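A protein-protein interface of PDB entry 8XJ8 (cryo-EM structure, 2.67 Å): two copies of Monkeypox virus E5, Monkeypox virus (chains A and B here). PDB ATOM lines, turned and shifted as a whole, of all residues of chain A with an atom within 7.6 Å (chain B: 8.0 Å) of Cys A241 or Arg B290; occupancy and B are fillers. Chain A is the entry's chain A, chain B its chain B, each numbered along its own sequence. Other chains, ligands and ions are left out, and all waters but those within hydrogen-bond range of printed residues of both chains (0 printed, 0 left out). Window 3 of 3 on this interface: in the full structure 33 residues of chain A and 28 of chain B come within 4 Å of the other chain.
The side-chain carboxylate (OD2) of Asp A238 is in salt-bridge range of the guanidinium group (NE) of Arg B290 (2.7 Å).
OH of Tyr A284 lies close to OD2 of Asp B292.
OD2 of Asp A238 sits at hydrogen-bond distance from SG of Cys A241.
O of Asp A238 lies within hydrogen-bond range of OG of Ser A244 (3.4 Å).
OD2 of Asp B250 is in salt-bridge range of NH2 of Arg B248 (3.1 Å).
The side-chain carboxylate (OD1) of Asp B289 is in hydrogen-bond range of the backbone NH (N) of Ser B249 (3.0 Å).
OG of Ser B249 sits close to N of Arg B290, 3.4 Å away.
The side-chain amino group (NZ) of Lys B253 lies within salt-bridge range of the side-chain carboxylate (OD2) of Asp B292.
Among the printed residues, merely in contact across the chains: Tyr A284 with Arg B290 (3.4 Å), Ser A242 with Asp B289 (3.5 Å), Cys A241 with Arg B290 (3.7 Å), Pro A237 with Asp B250 (3.8 Å), Cys A241 with Asp B289 (3.96 Å) and Asn A283 with Lys B253 (3.98 Å).
Of the printed residues of chain B, Asp A238 touches Arg B290.
Ala A240 touches none of the printed residues of chain B.
Cys A241 touches just these residues of chain B: Asp B289 (3.96 Å) and Arg B290 (3.7 Å).
Of the printed residues of chain B, Asn A283 touches Lys B253.
Val B287 touches none of the printed residues of chain A.
Arg B290 touches just these residues of chain A: Asp A238 (2.7 Å), Cys A241 (3.7 Å) and Tyr A284 (3.4 Å).
Of the printed residues of chain A, Asp B292 touches Tyr A284 (3.2 Å).
The nearest printed residue of chain B that does not touch Ser A242 is Arg B290 (5.3 Å).
Hydrophobic or aromatic side chains of chain A within 4 Å of the printed part of chain B: Pro A237 and Tyr A284.
Along chain A the printed residues that touch a printed residue of chain B span positions 237 to 284.
Of the 16 printed residues of chain B, 5 touch a printed residue of chain A.
Among the printed residues, Asp or Glu carboxylates within 4 Å of a Lys or Arg side-chain nitrogen of the other chain: Asp A238 with Arg B290.
No position is printed for both chains.
Of the 8 pairs that touch across the chains among the printed residues, none has its exchanged pair printed and touching as well.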
ATOM      1  N   PRO A 237     -26.360   4.641  24.059  1.00  0.00           N
ATOM      2  CA  PRO A 237     -25.105   5.225  23.581  1.00  0.00           C
ATOM      3  C   PRO A 237     -24.817   6.566  24.236  1.00  0.00           C
ATOM      4  O   PRO A 237     -25.706   7.246  24.754  1.00  0.00           O
ATOM      5  CB  PRO A 237     -25.347   5.389  22.078  1.00  0.00           C
ATOM      6  CG  PRO A 237     -26.822   5.587  21.983  1.00  0.00           C
ATOM      7  CD  PRO A 237     -27.400   4.657  23.016  1.00  0.00           C
ATOM      8  N   ASP A 238     -23.541   6.937  24.213  1.00  0.00           N
ATOM      9  CA  ASP A 238     -23.135   8.276  24.623  1.00  0.00           C
ATOM     10  C   ASP A 238     -23.617   9.267  23.571  1.00  0.00           C
ATOM     11  O   ASP A 238     -23.242   9.171  22.400  1.00  0.00           O
ATOM     12  CB  ASP A 238     -21.622   8.346  24.796  1.00  0.00           C
ATOM     13  CG  ASP A 238     -21.185   9.549  25.607  1.00  0.00           C
ATOM     14  OD1 ASP A 238     -22.057  10.213  26.205  1.00  0.00           O
ATOM     15  OD2 ASP A 238     -19.972   9.831  25.646  1.00  0.00           O
ATOM     16  N   PHE A 239     -24.449  10.218  23.984  1.00  0.00           N
ATOM     17  CA  PHE A 239     -25.133  11.088  23.038  1.00  0.00           C
ATOM     18  C   PHE A 239     -24.285  12.267  22.579  1.00  0.00           C
ATOM     19  O   PHE A 239     -24.746  13.045  21.738  1.00  0.00           O
ATOM     20  CB  PHE A 239     -26.437  11.597  23.656  1.00  0.00           C
ATOM     21  CG  PHE A 239     -27.445  10.515  23.915  1.00  0.00           C
ATOM     22  CD1 PHE A 239     -28.280  10.071  22.905  1.00  0.00           C
ATOM     23  CD2 PHE A 239     -27.554   9.940  25.169  1.00  0.00           C
ATOM     24  CE1 PHE A 239     -29.208   9.076  23.143  1.00  0.00           C
ATOM     25  CE2 PHE A 239     -28.479   8.945  25.412  1.00  0.00           C
ATOM     26  CZ  PHE A 239     -29.306   8.513  24.398  1.00  0.00           C
ATOM     27  N   ALA A 240     -23.065  12.421  23.101  1.00  0.00           N
ATOM     28  CA  ALA A 240     -22.230  13.558  22.750  1.00  0.00           C
ATOM     29  C   ALA A 240     -21.020  13.056  21.985  1.00  0.00           C
ATOM     30  O   ALA A 240     -20.781  13.500  20.845  1.00  0.00           O
ATOM     31  CB  ALA A 240     -21.861  14.354  24.008  1.00  0.00           C
ATOM     32  N   CYS A 241     -20.224  12.139  22.541  1.00  0.00           N
ATOM     33  CA  CYS A 241     -18.981  11.742  21.887  1.00  0.00           C
ATOM     34  C   CYS A 241     -19.209  10.805  20.709  1.00  0.00           C
ATOM     35  O   CYS A 241     -18.323  10.672  19.858  1.00  0.00           O
ATOM     36  CB  CYS A 241     -18.043  11.083  22.902  1.00  0.00           C
ATOM     37  SG  CYS A 241     -17.872  11.990  24.457  1.00  0.00           S
ATOM     38  N   SER A 242     -20.367  10.152  20.636  1.00  0.00           N
ATOM     39  CA  SER A 242     -20.669   9.257  19.526  1.00  0.00           C
ATOM     40  C   SER A 242     -21.486   9.918  18.427  1.00  0.00           C
ATOM     41  O   SER A 242     -21.471   9.439  17.289  1.00  0.00           O
ATOM     42  CB  SER A 242     -21.413   8.016  20.030  1.00  0.00           C
ATOM     43  OG  SER A 242     -22.768   8.313  20.318  1.00  0.00           O
ATOM     44  N   GLY A 243     -22.190  11.004  18.735  1.00  0.00           N
ATOM     45  CA  GLY A 243     -23.000  11.693  17.749  1.00  0.00           C
ATOM     46  C   GLY A 243     -24.148  10.858  17.222  1.00  0.00           C
ATOM     47  O   GLY A 243     -24.401  10.833  16.013  1.00  0.00           O
ATOM     48  N   SER A 244     -24.852  10.174  18.116  1.00  0.00           N
ATOM     49  CA  SER A 244     -25.951   9.292  17.753  1.00  0.00           C
ATOM     50  C   SER A 244     -27.284  10.008  17.922  1.00  0.00           C
ATOM     51  O   SER A 244     -27.354  11.160  18.358  1.00  0.00           O
ATOM     52  CB  SER A 244     -25.923   8.012  18.597  1.00  0.00           C
ATOM     53  OG  SER A 244     -24.914   8.078  19.590  1.00  0.00           O
ATOM     54  N   ASN A 283     -25.088   3.077  31.209  1.00  0.00           N
ATOM     55  CA  ASN A 283     -23.850   3.645  31.723  1.00  0.00           C
ATOM     56  C   ASN A 283     -23.779   5.153  31.519  1.00  0.00           C
ATOM     57  O   ASN A 283     -22.850   5.788  32.026  1.00  0.00           O
ATOM     58  CB  ASN A 283     -22.635   2.989  31.054  1.00  0.00           C
ATOM     59  CG  ASN A 283     -22.475   1.528  31.425  1.00  0.00           C
ATOM     60  OD1 ASN A 283     -22.904   0.640  30.691  1.00  0.00           O
ATOM     61  ND2 ASN A 283     -21.849   1.272  32.566  1.00  0.00           N
ATOM     62  N   TYR A 284     -24.736   5.732  30.793  1.00  0.00           N
ATOM     63  CA  TYR A 284     -24.779   7.158  30.510  1.00  0.00           C
ATOM     64  C   TYR A 284     -26.192   7.668  30.743  1.00  0.00           C
ATOM     65  O   TYR A 284     -27.164   6.996  30.393  1.00  0.00           O
ATOM     66  CB  TYR A 284     -24.357   7.460  29.066  1.00  0.00           C
ATOM     67  CG  TYR A 284     -22.976   6.970  28.706  1.00  0.00           C
ATOM     68  CD1 TYR A 284     -21.844   7.627  29.166  1.00  0.00           C
ATOM     69  CD2 TYR A 284     -22.806   5.849  27.907  1.00  0.00           C
ATOM     70  CE1 TYR A 284     -20.581   7.180  28.839  1.00  0.00           C
ATOM     71  CE2 TYR A 284     -21.546   5.396  27.575  1.00  0.00           C
ATOM     72  CZ  TYR A 284     -20.438   6.065  28.045  1.00  0.00           C
ATOM     73  OH  TYR A 284     -19.180   5.620  27.717  1.00  0.00           O
ATOM     74  N   LYS B 246     -16.698   4.602  12.639  1.00  0.00           N
ATOM     75  CA  LYS B 246     -16.206   3.937  13.834  1.00  0.00           C
ATOM     76  C   LYS B 246     -17.104   2.748  14.174  1.00  0.00           C
ATOM     77  O   LYS B 246     -18.213   2.603  13.649  1.00  0.00           O
ATOM     78  CB  LYS B 246     -16.137   4.919  15.001  1.00  0.00           C
ATOM     79  CG  LYS B 246     -15.025   5.948  14.874  1.00  0.00           C
ATOM     80  CD  LYS B 246     -13.804   5.374  14.179  1.00  0.00           C
ATOM     81  CE  LYS B 246     -12.779   6.456  13.884  1.00  0.00           C
ATOM     82  NZ  LYS B 246     -13.358   7.552  13.059  1.00  0.00           N
ATOM     83  N   ILE B 247     -16.615   1.884  15.063  1.00  0.00           N
ATOM     84  CA  ILE B 247     -17.296   0.618  15.312  1.00  0.00           C
ATOM     85  C   ILE B 247     -18.664   0.867  15.937  1.00  0.00           C
ATOM     86  O   ILE B 247     -19.679   0.638  15.276  1.00  0.00           O
ATOM     87  CB  ILE B 247     -16.441  -0.320  16.184  1.00  0.00           C
ATOM     88  CG1 ILE B 247     -15.321  -0.931  15.342  1.00  0.00           C
ATOM     89  CG2 ILE B 247     -17.289  -1.434  16.776  1.00  0.00           C
ATOM     90  CD1 ILE B 247     -14.401  -1.829  16.118  1.00  0.00           C
ATOM     91  N   ARG B 248     -18.681   1.411  17.166  1.00  0.00           N
ATOM     92  CA  ARG B 248     -19.833   1.662  18.046  1.00  0.00           C
ATOM     93  C   ARG B 248     -19.647   0.921  19.364  1.00  0.00           C
ATOM     94  O   ARG B 248     -19.703  -0.311  19.402  1.00  0.00           O
ATOM     95  CB  ARG B 248     -21.186   1.257  17.448  1.00  0.00           C
ATOM     96  CG  ARG B 248     -21.871   2.348  16.644  1.00  0.00           C
ATOM     97  CD  ARG B 248     -23.079   1.802  15.903  1.00  0.00           C
ATOM     98  NE  ARG B 248     -24.291   1.865  16.710  1.00  0.00           N
ATOM     99  CZ  ARG B 248     -25.096   2.917  16.767  1.00  0.00           C
ATOM    100  NH1 ARG B 248     -24.853   4.012  16.068  1.00  0.00           N
ATOM    101  NH2 ARG B 248     -26.173   2.867  17.546  1.00  0.00           N
ATOM    102  N   SER B 249     -19.430   1.666  20.450  1.00  0.00           N
ATOM    103  CA  SER B 249     -19.227   1.034  21.750  1.00  0.00           C
ATOM    104  C   SER B 249     -20.487   0.336  22.244  1.00  0.00           C
ATOM    105  O   SER B 249     -20.398  -0.709  22.897  1.00  0.00           O
ATOM    106  CB  SER B 249     -18.763   2.076  22.767  1.00  0.00           C
ATOM    107  OG  SER B 249     -17.527   2.644  22.375  1.00  0.00           O
ATOM    108  N   ASP B 250     -21.663   0.893  21.950  1.00  0.00           N
ATOM    109  CA  ASP B 250     -22.900   0.294  22.442  1.00  0.00           C
ATOM    110  C   ASP B 250     -23.245  -0.987  21.694  1.00  0.00           C
ATOM    111  O   ASP B 250     -23.882  -1.877  22.264  1.00  0.00           O
ATOM    112  CB  ASP B 250     -24.051   1.295  22.341  1.00  0.00           C
ATOM    113  CG  ASP B 250     -24.168   1.914  20.965  1.00  0.00           C
ATOM    114  OD1 ASP B 250     -23.176   2.504  20.490  1.00  0.00           O
ATOM    115  OD2 ASP B 250     -25.256   1.812  20.359  1.00  0.00           O
ATOM    116  N   LYS B 253     -21.624  -3.913  23.470  1.00  0.00           N
ATOM    117  CA  LYS B 253     -22.251  -4.291  24.732  1.00  0.00           C
ATOM    118  C   LYS B 253     -23.538  -5.081  24.520  1.00  0.00           C
ATOM    119  O   LYS B 253     -23.878  -5.936  25.345  1.00  0.00           O
ATOM    120  CB  LYS B 253     -22.521  -3.042  25.568  1.00  0.00           C
ATOM    121  CG  LYS B 253     -21.265  -2.312  26.008  1.00  0.00           C
ATOM    122  CD  LYS B 253     -21.588  -1.171  26.953  1.00  0.00           C
ATOM    123  CE  LYS B 253     -21.123   0.161  26.389  1.00  0.00           C
ATOM    124  NZ  LYS B 253     -20.633   1.078  27.452  1.00  0.00           N
ATOM    125  N   VAL B 287     -10.913   0.435  16.157  1.00  0.00           N
ATOM    126  CA  VAL B 287     -11.070   1.802  16.635  1.00  0.00           C
ATOM    127  C   VAL B 287     -12.542   2.027  16.947  1.00  0.00           C
ATOM    128  O   VAL B 287     -13.411   1.715  16.125  1.00  0.00           O
ATOM    129  CB  VAL B 287     -10.562   2.829  15.606  1.00  0.00           C
ATOM    130  CG1 VAL B 287     -10.842   4.244  16.080  1.00  0.00           C
ATOM    131  CG2 VAL B 287      -9.076   2.636  15.353  1.00  0.00           C
ATOM    132  N   PHE B 288     -12.820   2.566  18.131  1.00  0.00           N
ATOM    133  CA  PHE B 288     -14.179   2.735  18.621  1.00  0.00           C
ATOM    134  C   PHE B 288     -14.527   4.214  18.725  1.00  0.00           C
ATOM    135  O   PHE B 288     -13.654   5.064  18.926  1.00  0.00           O
ATOM    136  CB  PHE B 288     -14.355   2.063  19.987  1.00  0.00           C
ATOM    137  CG  PHE B 288     -13.950   0.618  20.007  1.00  0.00           C
ATOM    138  CD1 PHE B 288     -14.860  -0.375  19.691  1.00  0.00           C
ATOM    139  CD2 PHE B 288     -12.655   0.253  20.337  1.00  0.00           C
ATOM    140  CE1 PHE B 288     -14.488  -1.703  19.707  1.00  0.00           C
ATOM    141  CE2 PHE B 288     -12.278  -1.074  20.353  1.00  0.00           C
ATOM    142  CZ  PHE B 288     -13.195  -2.053  20.037  1.00  0.00           C
ATOM    143  N   ASP B 289     -15.820   4.512  18.579  1.00  0.00           N
ATOM    144  CA  ASP B 289     -16.279   5.895  18.677  1.00  0.00           C
ATOM    145  C   ASP B 289     -16.120   6.446  20.089  1.00  0.00           C
ATOM    146  O   ASP B 289     -15.816   7.632  20.258  1.00  0.00           O
ATOM    147  CB  ASP B 289     -17.734   5.999  18.218  1.00  0.00           C
ATOM    148  CG  ASP B 289     -18.661   5.083  18.992  1.00  0.00           C
ATOM    149  OD1 ASP B 289     -18.170   4.290  19.822  1.00  0.00           O
ATOM    150  OD2 ASP B 289     -19.887   5.150  18.767  1.00  0.00           O
ATOM    151  N   ARG B 290     -16.324   5.613  21.106  1.00  0.00           N
ATOM    152  CA  ARG B 290     -16.162   6.021  22.492  1.00  0.00           C
ATOM    153  C   ARG B 290     -15.457   4.915  23.260  1.00  0.00           C
ATOM    154  O   ARG B 290     -15.727   3.730  23.045  1.00  0.00           O
ATOM    155  CB  ARG B 290     -17.514   6.344  23.141  1.00  0.00           C
ATOM    156  CG  ARG B 290     -17.440   6.635  24.629  1.00  0.00           C
ATOM    157  CD  ARG B 290     -17.271   8.119  24.892  1.00  0.00           C
ATOM    158  NE  ARG B 290     -17.749   8.498  26.215  1.00  0.00           N
ATOM    159  CZ  ARG B 290     -17.036   8.387  27.327  1.00  0.00           C
ATOM    160  NH1 ARG B 290     -15.802   7.914  27.314  1.00  0.00           N
ATOM    161  NH2 ARG B 290     -17.575   8.764  28.484  1.00  0.00           N
ATOM    162  N   ILE B 291     -14.550   5.304  24.152  1.00  0.00           N
ATOM    163  CA  ILE B 291     -13.800   4.375  24.988  1.00  0.00           C
ATOM    164  C   ILE B 291     -14.324   4.488  26.411  1.00  0.00           C
ATOM    165  O   ILE B 291     -14.441   5.596  26.950  1.00  0.00           O
ATOM    166  CB  ILE B 291     -12.289   4.656  24.930  1.00  0.00           C
ATOM    167  CG1 ILE B 291     -11.789   4.610  23.484  1.00  0.00           C
ATOM    168  CG2 ILE B 291     -11.531   3.656  25.776  1.00  0.00           C
ATOM    169  CD1 ILE B 291     -12.182   3.356  22.740  1.00  0.00           C
ATOM    170  N   ASP B 292     -14.638   3.346  27.018  1.00  0.00           N
ATOM    171  CA  ASP B 292     -15.217   3.323  28.353  1.00  0.00           C
ATOM    172  C   ASP B 292     -14.731   2.081  29.084  1.00  0.00           C
ATOM    173  O   ASP B 292     -14.259   1.121  28.472  1.00  0.00           O
ATOM    174  CB  ASP B 292     -16.749   3.352  28.297  1.00  0.00           C
ATOM    175  CG  ASP B 292     -17.373   3.772  29.611  1.00  0.00           C
ATOM    176  OD1 ASP B 292     -16.806   4.660  30.283  1.00  0.00           O
ATOM    177  OD2 ASP B 292     -18.430   3.215  29.974  1.00  0.00           O
ATOM    178  N   ASN B 293     -14.847   2.116  30.415  1.00  0.00           N
ATOM    179  CA  ASN B 293     -14.463   0.962  31.219  1.00  0.00           C
ATOM    180  C   ASN B 293     -15.351  -0.242  30.934  1.00  0.00           C
ATOM    181  O   ASN B 293     -14.904  -1.386  31.075  1.00  0.00           O
ATOM    182  CB  ASN B 293     -14.512   1.313  32.706  1.00  0.00           C
ATOM    183  CG  ASN B 293     -13.253   2.004  33.183  1.00  0.00           C
ATOM    184  OD1 ASN B 293     -12.267   2.099  32.453  1.00  0.00           O
ATOM    185  ND2 ASN B 293     -13.279   2.492  34.416  1.00  0.00           N
ATOM    186  N   LEU B 295     -16.452  -0.986  27.959  1.00  0.00           N
ATOM    187  CA  LEU B 295     -15.959  -1.534  26.700  1.00  0.00           C
ATOM    188  C   LEU B 295     -14.647  -2.287  26.891  1.00  0.00           C
ATOM    189  O   LEU B 295     -14.404  -3.295  26.218  1.00  0.00           O
ATOM    190  CB  LEU B 295     -15.792  -0.411  25.676  1.00  0.00           C
ATOM    191  CG  LEU B 295     -15.336  -0.797  24.268  1.00  0.00           C
ATOM    192  CD1 LEU B 295     -16.514  -1.261  23.434  1.00  0.00           C
ATOM    193  CD2 LEU B 295     -14.636   0.373  23.601  1.00  0.00           C
ATOM    194  N   MET B 296     -13.792  -1.818  27.804  1.00  0.00           N
ATOM    195  CA  MET B 296     -12.519  -2.484  28.060  1.00  0.00           C
ATOM    196  C   MET B 296     -12.696  -3.894  28.604  1.00  0.00           C
ATOM    197  O   MET B 296     -11.796  -4.726  28.442  1.00  0.00           O
ATOM    198  CB  MET B 296     -11.683  -1.667  29.046  1.00  0.00           C
ATOM    199  CG  MET B 296     -10.751  -0.655  28.409  1.00  0.00           C
ATOM    200  SD  MET B 296     -10.675   0.879  29.351  1.00  0.00           S
ATOM    201  CE  MET B 296      -9.663   1.886  28.275  1.00  0.00           C
ATOM    202  N   ASP B 373      -5.976   2.261  21.850  1.00  0.00           N
ATOM    203  CA  ASP B 373      -6.981   3.151  22.417  1.00  0.00           C
ATOM    204  C   ASP B 373      -7.128   2.911  23.916  1.00  0.00           C
ATOM    205  O   ASP B 373      -7.280   3.852  24.694  1.00  0.00           O
ATOM    206  CB  ASP B 373      -8.327   2.958  21.719  1.00  0.00           C
ATOM    207  CG  ASP B 373      -8.269   3.280  20.241  1.00  0.00           C
ATOM    208  OD1 ASP B 373      -7.199   3.078  19.630  1.00  0.00           O
ATOM    209  OD2 ASP B 373      -9.293   3.734  19.689  1.00  0.00           O
